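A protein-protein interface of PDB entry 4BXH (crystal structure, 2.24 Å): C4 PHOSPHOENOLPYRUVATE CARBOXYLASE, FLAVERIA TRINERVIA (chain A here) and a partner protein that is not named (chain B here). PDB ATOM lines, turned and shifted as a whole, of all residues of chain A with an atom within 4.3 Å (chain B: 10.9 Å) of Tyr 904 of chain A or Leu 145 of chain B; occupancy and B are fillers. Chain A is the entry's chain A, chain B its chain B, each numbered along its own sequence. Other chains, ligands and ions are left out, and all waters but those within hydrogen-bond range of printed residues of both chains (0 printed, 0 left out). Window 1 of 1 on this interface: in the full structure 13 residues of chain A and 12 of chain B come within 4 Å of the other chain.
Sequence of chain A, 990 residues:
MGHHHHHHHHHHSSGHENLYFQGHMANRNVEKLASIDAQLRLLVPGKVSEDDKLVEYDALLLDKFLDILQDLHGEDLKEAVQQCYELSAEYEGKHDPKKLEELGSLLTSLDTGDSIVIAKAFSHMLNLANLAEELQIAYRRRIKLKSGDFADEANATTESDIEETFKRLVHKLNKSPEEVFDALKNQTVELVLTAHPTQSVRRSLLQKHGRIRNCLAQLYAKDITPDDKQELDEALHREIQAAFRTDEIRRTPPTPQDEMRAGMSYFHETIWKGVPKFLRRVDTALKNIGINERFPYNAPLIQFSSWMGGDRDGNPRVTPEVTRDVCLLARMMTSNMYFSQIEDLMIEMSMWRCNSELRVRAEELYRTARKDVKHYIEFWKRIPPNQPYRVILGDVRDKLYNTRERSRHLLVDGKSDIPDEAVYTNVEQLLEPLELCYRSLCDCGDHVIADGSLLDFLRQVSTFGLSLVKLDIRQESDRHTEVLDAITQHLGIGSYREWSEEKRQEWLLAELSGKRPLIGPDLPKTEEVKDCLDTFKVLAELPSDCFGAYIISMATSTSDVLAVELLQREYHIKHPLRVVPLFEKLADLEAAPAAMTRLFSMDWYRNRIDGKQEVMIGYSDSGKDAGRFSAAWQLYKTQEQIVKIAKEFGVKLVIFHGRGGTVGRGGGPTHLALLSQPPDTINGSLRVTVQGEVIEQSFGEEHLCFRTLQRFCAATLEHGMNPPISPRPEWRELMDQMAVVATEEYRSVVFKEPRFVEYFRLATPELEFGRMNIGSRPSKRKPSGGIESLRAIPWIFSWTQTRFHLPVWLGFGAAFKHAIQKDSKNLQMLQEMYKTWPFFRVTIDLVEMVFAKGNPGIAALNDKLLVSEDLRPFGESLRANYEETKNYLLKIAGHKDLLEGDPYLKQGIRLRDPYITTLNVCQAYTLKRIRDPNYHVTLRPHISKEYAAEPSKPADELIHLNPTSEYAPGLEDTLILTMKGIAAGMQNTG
The side-chain hydroxyl (OH) of Tyr 904 of chain A lies close to the side-chain amino group (NZ) of Lys 144 of chain B, at 3.0 Å.
Among the printed residues, merely in contact across the chains: Lys 47 of chain A with Lys 144 of chain B, Tyr 904 of chain A with Leu 145 of chain B, Pro 903 of chain A with Leu 145 of chain B and Lys 47 of chain A with Leu 145 of chain B.
Of the printed residues of chain B, Lys 47 of chain A touches Lys 144 and Leu 145.
Asp 902 of chain A touches none of the printed residues of chain B.
Of chain B, only Leu 145 comes within 4 Å of Pro 903 of chain A.
Tyr 904 of chain A touches just these residues of chain B: Lys 144 and Leu 145.
Leu 905 of chain A touches none of the printed residues of chain B.
No residue of chain B comes within 4 Å of Gln 907 of chain A.
Gly 908 of chain A touches none of the printed residues of chain B.
Of the printed residues of chain A, Lys 144 of chain B touches Lys 47 and Tyr 904.
Of the printed residues of chain A, Leu 145 of chain B touches Lys 47, Pro 903 and Tyr 904.
The nearest printed residue of chain B that does not touch Tyr 904 of chain A is Lys 146 of chain B (8.3 Å).
The nearest printed residue of chain A that does not touch Leu 145 of chain B is Asp 902 of chain A (6.5 Å).
Of the 9 printed residues of chain A, 3 touch a printed residue of chain B.
Along chain A the printed residues that touch a printed residue of chain B span positions 47 to 904.
Hydrophobic or aromatic side chains of chain B that line the printed part of chain A: Leu 145.
Among the printed residues, 5 pairs touch across the chains.
Among the printed residues, no Asp or Glu carboxylate lies within 4 Å of a Lys or Arg side-chain nitrogen of the other chain.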
ATOM      1  N   LYS A  47       2.357 -18.813 -11.542  1.00  0.00           N
ATOM      2  CA  LYS A  47       2.388 -18.041 -12.800  1.00  0.00           C
ATOM      3  C   LYS A  47       0.978 -17.932 -13.426  1.00  0.00           C
ATOM      4  O   LYS A  47       0.676 -18.528 -14.463  1.00  0.00           O
ATOM      5  CB  LYS A  47       3.508 -18.564 -13.762  1.00  0.00           C
ATOM      6  CG  LYS A  47       3.574 -20.059 -14.146  1.00  0.00           C
ATOM      7  CD  LYS A  47       3.316 -21.133 -13.066  1.00  0.00           C
ATOM      8  CE  LYS A  47       4.178 -21.056 -11.798  1.00  0.00           C
ATOM      9  NZ  LYS A  47       5.045 -22.233 -11.515  1.00  0.00           N
ATOM     10  N   ARG A 140      -9.139 -27.063 -15.170  1.00  0.00           N
ATOM     11  CA  ARG A 140      -7.767 -26.796 -15.572  1.00  0.00           C
ATOM     12  C   ARG A 140      -7.511 -27.214 -17.068  1.00  0.00           C
ATOM     13  O   ARG A 140      -7.835 -28.342 -17.495  1.00  0.00           O
ATOM     14  CB  ARG A 140      -6.840 -27.531 -14.598  1.00  0.00           C
ATOM     15  CG  ARG A 140      -5.387 -27.462 -14.948  1.00  0.00           C
ATOM     16  CD  ARG A 140      -4.640 -26.397 -14.215  1.00  0.00           C
ATOM     17  NE  ARG A 140      -4.648 -26.484 -12.748  1.00  0.00           N
ATOM     18  CZ  ARG A 140      -4.330 -25.409 -12.008  1.00  0.00           C
ATOM     19  NH1 ARG A 140      -4.031 -24.280 -12.647  1.00  0.00           N
ATOM     20  NH2 ARG A 140      -4.311 -25.419 -10.663  1.00  0.00           N
ATOM     21  N   ASP A 902       5.445 -31.073  -9.591  1.00  0.00           N
ATOM     22  CA  ASP A 902       4.025 -30.987  -9.655  1.00  0.00           C
ATOM     23  C   ASP A 902       3.469 -29.756  -8.969  1.00  0.00           C
ATOM     24  O   ASP A 902       2.876 -29.830  -7.943  1.00  0.00           O
ATOM     25  CB  ASP A 902       3.529 -32.255  -9.003  1.00  0.00           C
ATOM     26  CG  ASP A 902       2.077 -32.562  -9.314  1.00  0.00           C
ATOM     27  OD1 ASP A 902       1.301 -31.698  -9.873  1.00  0.00           O
ATOM     28  OD2 ASP A 902       1.707 -33.711  -8.961  1.00  0.00           O
ATOM     29  N   PRO A 903       3.631 -28.601  -9.558  1.00  0.00           N
ATOM     30  CA  PRO A 903       3.258 -27.380  -8.873  1.00  0.00           C
ATOM     31  C   PRO A 903       1.755 -27.222  -8.563  1.00  0.00           C
ATOM     32  O   PRO A 903       1.409 -26.553  -7.609  1.00  0.00           O
ATOM     33  CB  PRO A 903       3.717 -26.279  -9.854  1.00  0.00           C
ATOM     34  CG  PRO A 903       3.911 -26.959 -11.160  1.00  0.00           C
ATOM     35  CD  PRO A 903       4.366 -28.329 -10.807  1.00  0.00           C
ATOM     36  N   TYR A 904       0.861 -27.820  -9.343  1.00  0.00           N
ATOM     37  CA  TYR A 904      -0.596 -27.709  -9.077  1.00  0.00           C
ATOM     38  C   TYR A 904      -0.978 -28.474  -7.822  1.00  0.00           C
ATOM     39  O   TYR A 904      -1.731 -27.973  -6.956  1.00  0.00           O
ATOM     40  CB  TYR A 904      -1.415 -28.168 -10.285  1.00  0.00           C
ATOM     41  CG  TYR A 904      -1.172 -27.337 -11.494  1.00  0.00           C
ATOM     42  CD1 TYR A 904      -1.068 -25.941 -11.396  1.00  0.00           C
ATOM     43  CD2 TYR A 904      -1.084 -27.913 -12.753  1.00  0.00           C
ATOM     44  CE1 TYR A 904      -0.862 -25.151 -12.515  1.00  0.00           C
ATOM     45  CE2 TYR A 904      -0.870 -27.134 -13.891  1.00  0.00           C
ATOM     46  CZ  TYR A 904      -0.771 -25.744 -13.773  1.00  0.00           C
ATOM     47  OH  TYR A 904      -0.545 -24.939 -14.908  1.00  0.00           O
ATOM     48  N   LEU A 905      -0.352 -29.619  -7.635  1.00  0.00           N
ATOM     49  CA  LEU A 905      -0.546 -30.416  -6.409  1.00  0.00           C
ATOM     50  C   LEU A 905       0.054 -29.674  -5.223  1.00  0.00           C
ATOM     51  O   LEU A 905      -0.518 -29.636  -4.135  1.00  0.00           O
ATOM     52  CB  LEU A 905       0.097 -31.774  -6.559  1.00  0.00           C
ATOM     53  CG  LEU A 905      -0.058 -32.668  -5.315  1.00  0.00           C
ATOM     54  CD1 LEU A 905      -1.496 -33.113  -5.054  1.00  0.00           C
ATOM     55  CD2 LEU A 905       0.830 -33.877  -5.476  1.00  0.00           C
ATOM     56  N   LYS A 906       1.222 -29.093  -5.411  1.00  0.00           N
ATOM     57  CA  LYS A 906       1.845 -28.355  -4.312  1.00  0.00           C
ATOM     58  C   LYS A 906       0.993 -27.174  -3.940  1.00  0.00           C
ATOM     59  O   LYS A 906       0.824 -26.872  -2.769  1.00  0.00           O
ATOM     60  CB  LYS A 906       3.215 -27.865  -4.713  1.00  0.00           C
ATOM     61  CG  LYS A 906       4.068 -27.206  -3.644  1.00  0.00           C
ATOM     62  CD  LYS A 906       5.393 -26.802  -4.301  1.00  0.00           C
ATOM     63  CE  LYS A 906       6.285 -25.962  -3.406  1.00  0.00           C
ATOM     64  NZ  LYS A 906       7.207 -26.812  -2.595  1.00  0.00           N
ATOM     65  N   GLN A 907       0.457 -26.502  -4.925  1.00  0.00           N
ATOM     66  CA  GLN A 907      -0.375 -25.392  -4.643  1.00  0.00           C
ATOM     67  C   GLN A 907      -1.594 -25.821  -3.776  1.00  0.00           C
ATOM     68  O   GLN A 907      -1.939 -25.151  -2.799  1.00  0.00           O
ATOM     69  CB  GLN A 907      -0.843 -24.732  -5.932  1.00  0.00           C
ATOM     70  CG  GLN A 907      -1.790 -23.568  -5.649  1.00  0.00           C
ATOM     71  CD  GLN A 907      -2.393 -22.943  -6.872  1.00  0.00           C
ATOM     72  OE1 GLN A 907      -2.270 -21.750  -7.067  1.00  0.00           O
ATOM     73  NE2 GLN A 907      -3.057 -23.743  -7.700  1.00  0.00           N
ATOM     74  N   GLY A 908      -2.212 -26.954  -4.099  1.00  0.00           N
ATOM     75  CA  GLY A 908      -3.421 -27.375  -3.397  1.00  0.00           C
ATOM     76  C   GLY A 908      -3.117 -27.674  -1.934  1.00  0.00           C
ATOM     77  O   GLY A 908      -3.863 -27.249  -1.018  1.00  0.00           O
ATOM     78  N   ARG B 141       1.671 -19.592 -28.767  1.00  0.00           N
ATOM     79  CA  ARG B 141       1.646 -19.509 -27.298  1.00  0.00           C
ATOM     80  C   ARG B 141       2.842 -20.226 -26.653  1.00  0.00           C
ATOM     81  O   ARG B 141       3.124 -21.355 -26.975  1.00  0.00           O
ATOM     82  CB  ARG B 141       0.331 -20.138 -26.777  1.00  0.00           C
ATOM     83  CG  ARG B 141       0.015 -19.847 -25.310  1.00  0.00           C
ATOM     84  CD  ARG B 141      -0.796 -20.935 -24.546  1.00  0.00           C
ATOM     85  NE  ARG B 141      -2.260 -20.794 -24.615  1.00  0.00           N
ATOM     86  CZ  ARG B 141      -3.026 -21.143 -25.660  1.00  0.00           C
ATOM     87  NH1 ARG B 141      -2.497 -21.652 -26.767  1.00  0.00           N
ATOM     88  NH2 ARG B 141      -4.344 -20.981 -25.611  1.00  0.00           N
ATOM     89  N   ARG B 142       3.470 -19.580 -25.676  1.00  0.00           N
ATOM     90  CA  ARG B 142       4.465 -20.187 -24.789  1.00  0.00           C
ATOM     91  C   ARG B 142       3.867 -21.199 -23.868  1.00  0.00           C
ATOM     92  O   ARG B 142       2.747 -21.021 -23.377  1.00  0.00           O
ATOM     93  CB  ARG B 142       5.139 -19.080 -23.931  1.00  0.00           C
ATOM     94  CG  ARG B 142       5.849 -17.992 -24.794  1.00  0.00           C
ATOM     95  CD  ARG B 142       7.268 -18.396 -25.008  1.00  0.00           C
ATOM     96  NE  ARG B 142       8.026 -18.251 -23.752  1.00  0.00           N
ATOM     97  CZ  ARG B 142       9.141 -18.931 -23.442  1.00  0.00           C
ATOM     98  NH1 ARG B 142       9.664 -19.883 -24.280  1.00  0.00           N
ATOM     99  NH2 ARG B 142       9.705 -18.682 -22.262  1.00  0.00           N
ATOM    100  N   ILE B 143       4.554 -22.297 -23.657  1.00  0.00           N
ATOM    101  CA  ILE B 143       4.128 -23.288 -22.667  1.00  0.00           C
ATOM    102  C   ILE B 143       4.410 -22.708 -21.261  1.00  0.00           C
ATOM    103  O   ILE B 143       5.462 -22.201 -20.992  1.00  0.00           O
ATOM    104  CB  ILE B 143       4.859 -24.644 -22.824  1.00  0.00           C
ATOM    105  CG1 ILE B 143       4.559 -25.261 -24.229  1.00  0.00           C
ATOM    106  CG2 ILE B 143       4.446 -25.645 -21.741  1.00  0.00           C
ATOM    107  CD1 ILE B 143       3.091 -25.303 -24.629  1.00  0.00           C
ATOM    108  N   LYS B 144       3.431 -22.789 -20.388  1.00  0.00           N
ATOM    109  CA  LYS B 144       3.512 -22.146 -19.101  1.00  0.00           C
ATOM    110  C   LYS B 144       4.412 -22.964 -18.172  1.00  0.00           C
ATOM    111  O   LYS B 144       5.377 -22.457 -17.689  1.00  0.00           O
ATOM    112  CB  LYS B 144       2.074 -21.981 -18.596  1.00  0.00           C
ATOM    113  CG  LYS B 144       1.945 -21.196 -17.311  1.00  0.00           C
ATOM    114  CD  LYS B 144       0.486 -21.108 -16.837  1.00  0.00           C
ATOM    115  CE  LYS B 144       0.055 -22.306 -15.984  1.00  0.00           C
ATOM    116  NZ  LYS B 144      -1.096 -21.982 -15.095  1.00  0.00           N
ATOM    117  N   LEU B 145       4.144 -24.255 -18.007  1.00  0.00           N
ATOM    118  CA  LEU B 145       4.950 -25.113 -17.151  1.00  0.00           C
ATOM    119  C   LEU B 145       5.956 -25.936 -17.948  1.00  0.00           C
ATOM    120  O   LEU B 145       5.583 -26.937 -18.592  1.00  0.00           O
ATOM    121  CB  LEU B 145       4.074 -26.110 -16.448  1.00  0.00           C
ATOM    122  CG  LEU B 145       3.178 -25.579 -15.363  1.00  0.00           C
ATOM    123  CD1 LEU B 145       2.548 -26.811 -14.713  1.00  0.00           C
ATOM    124  CD2 LEU B 145       3.974 -24.734 -14.365  1.00  0.00           C
ATOM    125  N   LYS B 146       7.227 -25.564 -17.877  1.00  0.00           N
ATOM    126  CA  LYS B 146       8.243 -26.273 -18.662  1.00  0.00           C
ATOM    127  C   LYS B 146       8.734 -27.507 -17.832  1.00  0.00           C
ATOM    128  O   LYS B 146       8.894 -27.409 -16.603  1.00  0.00           O
ATOM    129  CB  LYS B 146       9.333 -25.260 -19.140  1.00  0.00           C
ATOM    130  CG  LYS B 146       8.764 -24.039 -19.968  1.00  0.00           C
ATOM    131  CD  LYS B 146       9.651 -22.749 -19.947  1.00  0.00           C
ATOM    132  CE  LYS B 146       9.226 -21.642 -20.960  1.00  0.00           C
ATOM    133  NZ  LYS B 146       8.013 -21.745 -21.989  1.00  0.00           N
ATOM    134  N   SER B 147       8.880 -28.681 -18.481  1.00  0.00           N
ATOM    135  CA  SER B 147       9.297 -29.940 -17.793  1.00  0.00           C
ATOM    136  C   SER B 147      10.714 -29.910 -17.193  1.00  0.00           C
ATOM    137  O   SER B 147      11.070 -30.810 -16.454  1.00  0.00           O
ATOM    138  CB  SER B 147       9.165 -31.186 -18.723  1.00  0.00           C
ATOM    139  OG  SER B 147      10.315 -31.396 -19.575  1.00  0.00           O
ATOM    140  N   GLY B 148      11.523 -28.905 -17.515  1.00  0.00           N
ATOM    141  CA  GLY B 148      12.900 -28.846 -17.011  1.00  0.00           C
ATOM    142  C   GLY B 148      13.960 -29.641 -17.800  1.00  0.00           C
ATOM    143  O   GLY B 148      15.114 -29.280 -17.749  1.00  0.00           O
ATOM    144  N   ASP B 149      13.582 -30.701 -18.525  1.00  0.00           N
ATOM    145  CA  ASP B 149      14.505 -31.414 -19.430  1.00  0.00           C
ATOM    146  C   ASP B 149      15.225 -30.443 -20.462  1.00  0.00           C
ATOM    147  O   ASP B 149      14.612 -29.466 -20.942  1.00  0.00           O
ATOM    148  CB  ASP B 149      13.751 -32.559 -20.163  1.00  0.00           C
ATOM    149  CG  ASP B 149      14.728 -33.545 -20.926  1.00  0.00           C
ATOM    150  OD1 ASP B 149      15.254 -33.252 -22.049  1.00  0.00           O
ATOM    151  OD2 ASP B 149      14.998 -34.630 -20.368  1.00  0.00           O
ATOM    152  N   ALA B 151      15.731 -30.846 -23.394  1.00  0.00           N
ATOM    153  CA  ALA B 151      15.009 -30.864 -24.660  1.00  0.00           C
ATOM    154  C   ALA B 151      14.047 -29.686 -24.840  1.00  0.00           C
ATOM    155  O   ALA B 151      13.708 -29.350 -25.957  1.00  0.00           O
ATOM    156  CB  ALA B 151      14.278 -32.180 -24.867  1.00  0.00           C
ATOM    157  N   ASP B 152      13.586 -29.080 -23.749  1.00  0.00           N
ATOM    158  CA  ASP B 152      12.730 -27.905 -23.842  1.00  0.00           C
ATOM    159  C   ASP B 152      13.404 -26.735 -24.557  1.00  0.00           C
ATOM    160  O   ASP B 152      12.715 -25.791 -24.952  1.00  0.00           O
ATOM    161  CB  ASP B 152      12.427 -27.390 -22.429  1.00  0.00           C
ATOM    162  CG  ASP B 152      11.526 -28.292 -21.657  1.00  0.00           C
ATOM    163  OD1 ASP B 152      10.865 -29.144 -22.295  1.00  0.00           O
ATOM    164  OD2 ASP B 152      11.499 -28.140 -20.401  1.00  0.00           O
ATOM    165  N   GLU B 153      14.745 -26.711 -24.512  1.00  0.00           N
ATOM    166  CA  GLU B 153      15.518 -25.592 -25.062  1.00  0.00           C
ATOM    167  C   GLU B 153      15.673 -25.745 -26.574  1.00  0.00           C
ATOM    168  O   GLU B 153      16.260 -24.889 -27.239  1.00  0.00           O
ATOM    169  CB  GLU B 153      16.869 -25.462 -24.401  1.00  0.00           C
ATOM    170  CG  GLU B 153      16.823 -25.385 -22.876  1.00  0.00           C
ATOM    171  CD  GLU B 153      16.195 -24.102 -22.381  1.00  0.00           C
ATOM    172  OE1 GLU B 153      16.007 -23.175 -23.155  1.00  0.00           O
ATOM    173  OE2 GLU B 153      15.914 -24.012 -21.187  1.00  0.00           O
ATOM    174  N   THR B 157       8.579 -22.579 -28.141  1.00  0.00           N
ATOM    175  CA  THR B 157       7.428 -22.483 -27.229  1.00  0.00           C
ATOM    176  C   THR B 157       7.812 -22.880 -25.827  1.00  0.00           C
ATOM    177  O   THR B 157       7.135 -22.480 -24.894  1.00  0.00           O
ATOM    178  CB  THR B 157       6.270 -23.381 -27.663  1.00  0.00           C
ATOM    179  OG1 THR B 157       6.696 -24.732 -27.584  1.00  0.00           O
ATOM    180  CG2 THR B 157       5.873 -23.075 -29.113  1.00  0.00           C
ATOM    181  N   THR B 158       8.892 -23.672 -25.682  1.00  0.00           N
ATOM    182  CA  THR B 158       9.328 -24.156 -24.394  1.00  0.00           C
ATOM    183  C   THR B 158      10.661 -23.577 -23.894  1.00  0.00           C
ATOM    184  O   THR B 158      10.966 -23.739 -22.717  1.00  0.00           O
ATOM    185  CB  THR B 158       9.439 -25.685 -24.322  1.00  0.00           C
ATOM    186  OG1 THR B 158      10.276 -26.172 -25.388  1.00  0.00           O
ATOM    187  CG2 THR B 158       8.055 -26.336 -24.380  1.00  0.00           C
ATOM    188  N   GLU B 159      11.474 -22.959 -24.740  1.00  0.00           N
ATOM    189  CA  GLU B 159      12.800 -22.541 -24.303  1.00  0.00           C
ATOM    190  C   GLU B 159      12.812 -21.500 -23.163  1.00  0.00           C
ATOM    191  O   GLU B 159      11.890 -20.730 -22.981  1.00  0.00           O
ATOM    192  CB  GLU B 159      13.603 -21.985 -25.456  1.00  0.00           C
ATOM    193  CG  GLU B 159      13.164 -20.608 -25.927  1.00  0.00           C
ATOM    194  CD  GLU B 159      13.859 -20.147 -27.220  1.00  0.00           C
ATOM    195  OE1 GLU B 159      15.061 -20.465 -27.493  1.00  0.00           O
ATOM    196  OE2 GLU B 159      13.199 -19.410 -27.971  1.00  0.00           O
ATOM    197  N   SER B 160      13.895 -21.423 -22.434  1.00  0.00           N
ATOM    198  CA  SER B 160      13.990 -20.478 -21.320  1.00  0.00           C
ATOM    199  C   SER B 160      14.241 -19.107 -21.926  1.00  0.00           C
ATOM    200  O   SER B 160      15.104 -18.943 -22.771  1.00  0.00           O
ATOM    201  CB  SER B 160      15.147 -20.857 -20.411  1.00  0.00           C
ATOM    202  OG  SER B 160      14.948 -22.169 -19.957  1.00  0.00           O
ATOM    203  N   GLU B 164      14.098 -16.630 -16.946  1.00  0.00           N
ATOM    204  CA  GLU B 164      14.049 -18.014 -16.567  1.00  0.00           C
ATOM    205  C   GLU B 164      15.458 -18.595 -16.562  1.00  0.00           C
ATOM    206  O   GLU B 164      15.791 -19.386 -15.698  1.00  0.00           O
ATOM    207  CB  GLU B 164      13.163 -18.844 -17.536  1.00  0.00           C
ATOM    208  CG  GLU B 164      11.684 -18.517 -17.459  1.00  0.00           C
ATOM    209  CD  GLU B 164      10.870 -19.021 -18.682  1.00  0.00           C
ATOM    210  OE1 GLU B 164      11.336 -19.129 -19.805  1.00  0.00           O
ATOM    211  OE2 GLU B 164       9.728 -19.331 -18.483  1.00  0.00           O
ATOM    212  N   ARG B 168      17.058 -20.217 -13.138  1.00  0.00           N
ATOM    213  CA  ARG B 168      17.649 -21.551 -13.037  1.00  0.00           C
ATOM    214  C   ARG B 168      19.080 -21.419 -12.473  1.00  0.00           C
ATOM    215  O   ARG B 168      19.522 -22.276 -11.726  1.00  0.00           O
ATOM    216  CB  ARG B 168      17.645 -22.302 -14.364  1.00  0.00           C
ATOM    217  CG  ARG B 168      18.314 -23.718 -14.405  1.00  0.00           C
ATOM    218  CD  ARG B 168      18.700 -24.100 -15.884  1.00  0.00           C
ATOM    219  NE  ARG B 168      17.478 -23.929 -16.566  1.00  0.00           N
ATOM    220  CZ  ARG B 168      17.136 -23.212 -17.612  1.00  0.00           C
ATOM    221  NH1 ARG B 168      17.923 -22.733 -18.554  1.00  0.00           N
ATOM    222  NH2 ARG B 168      15.824 -23.175 -17.771  1.00  0.00           N
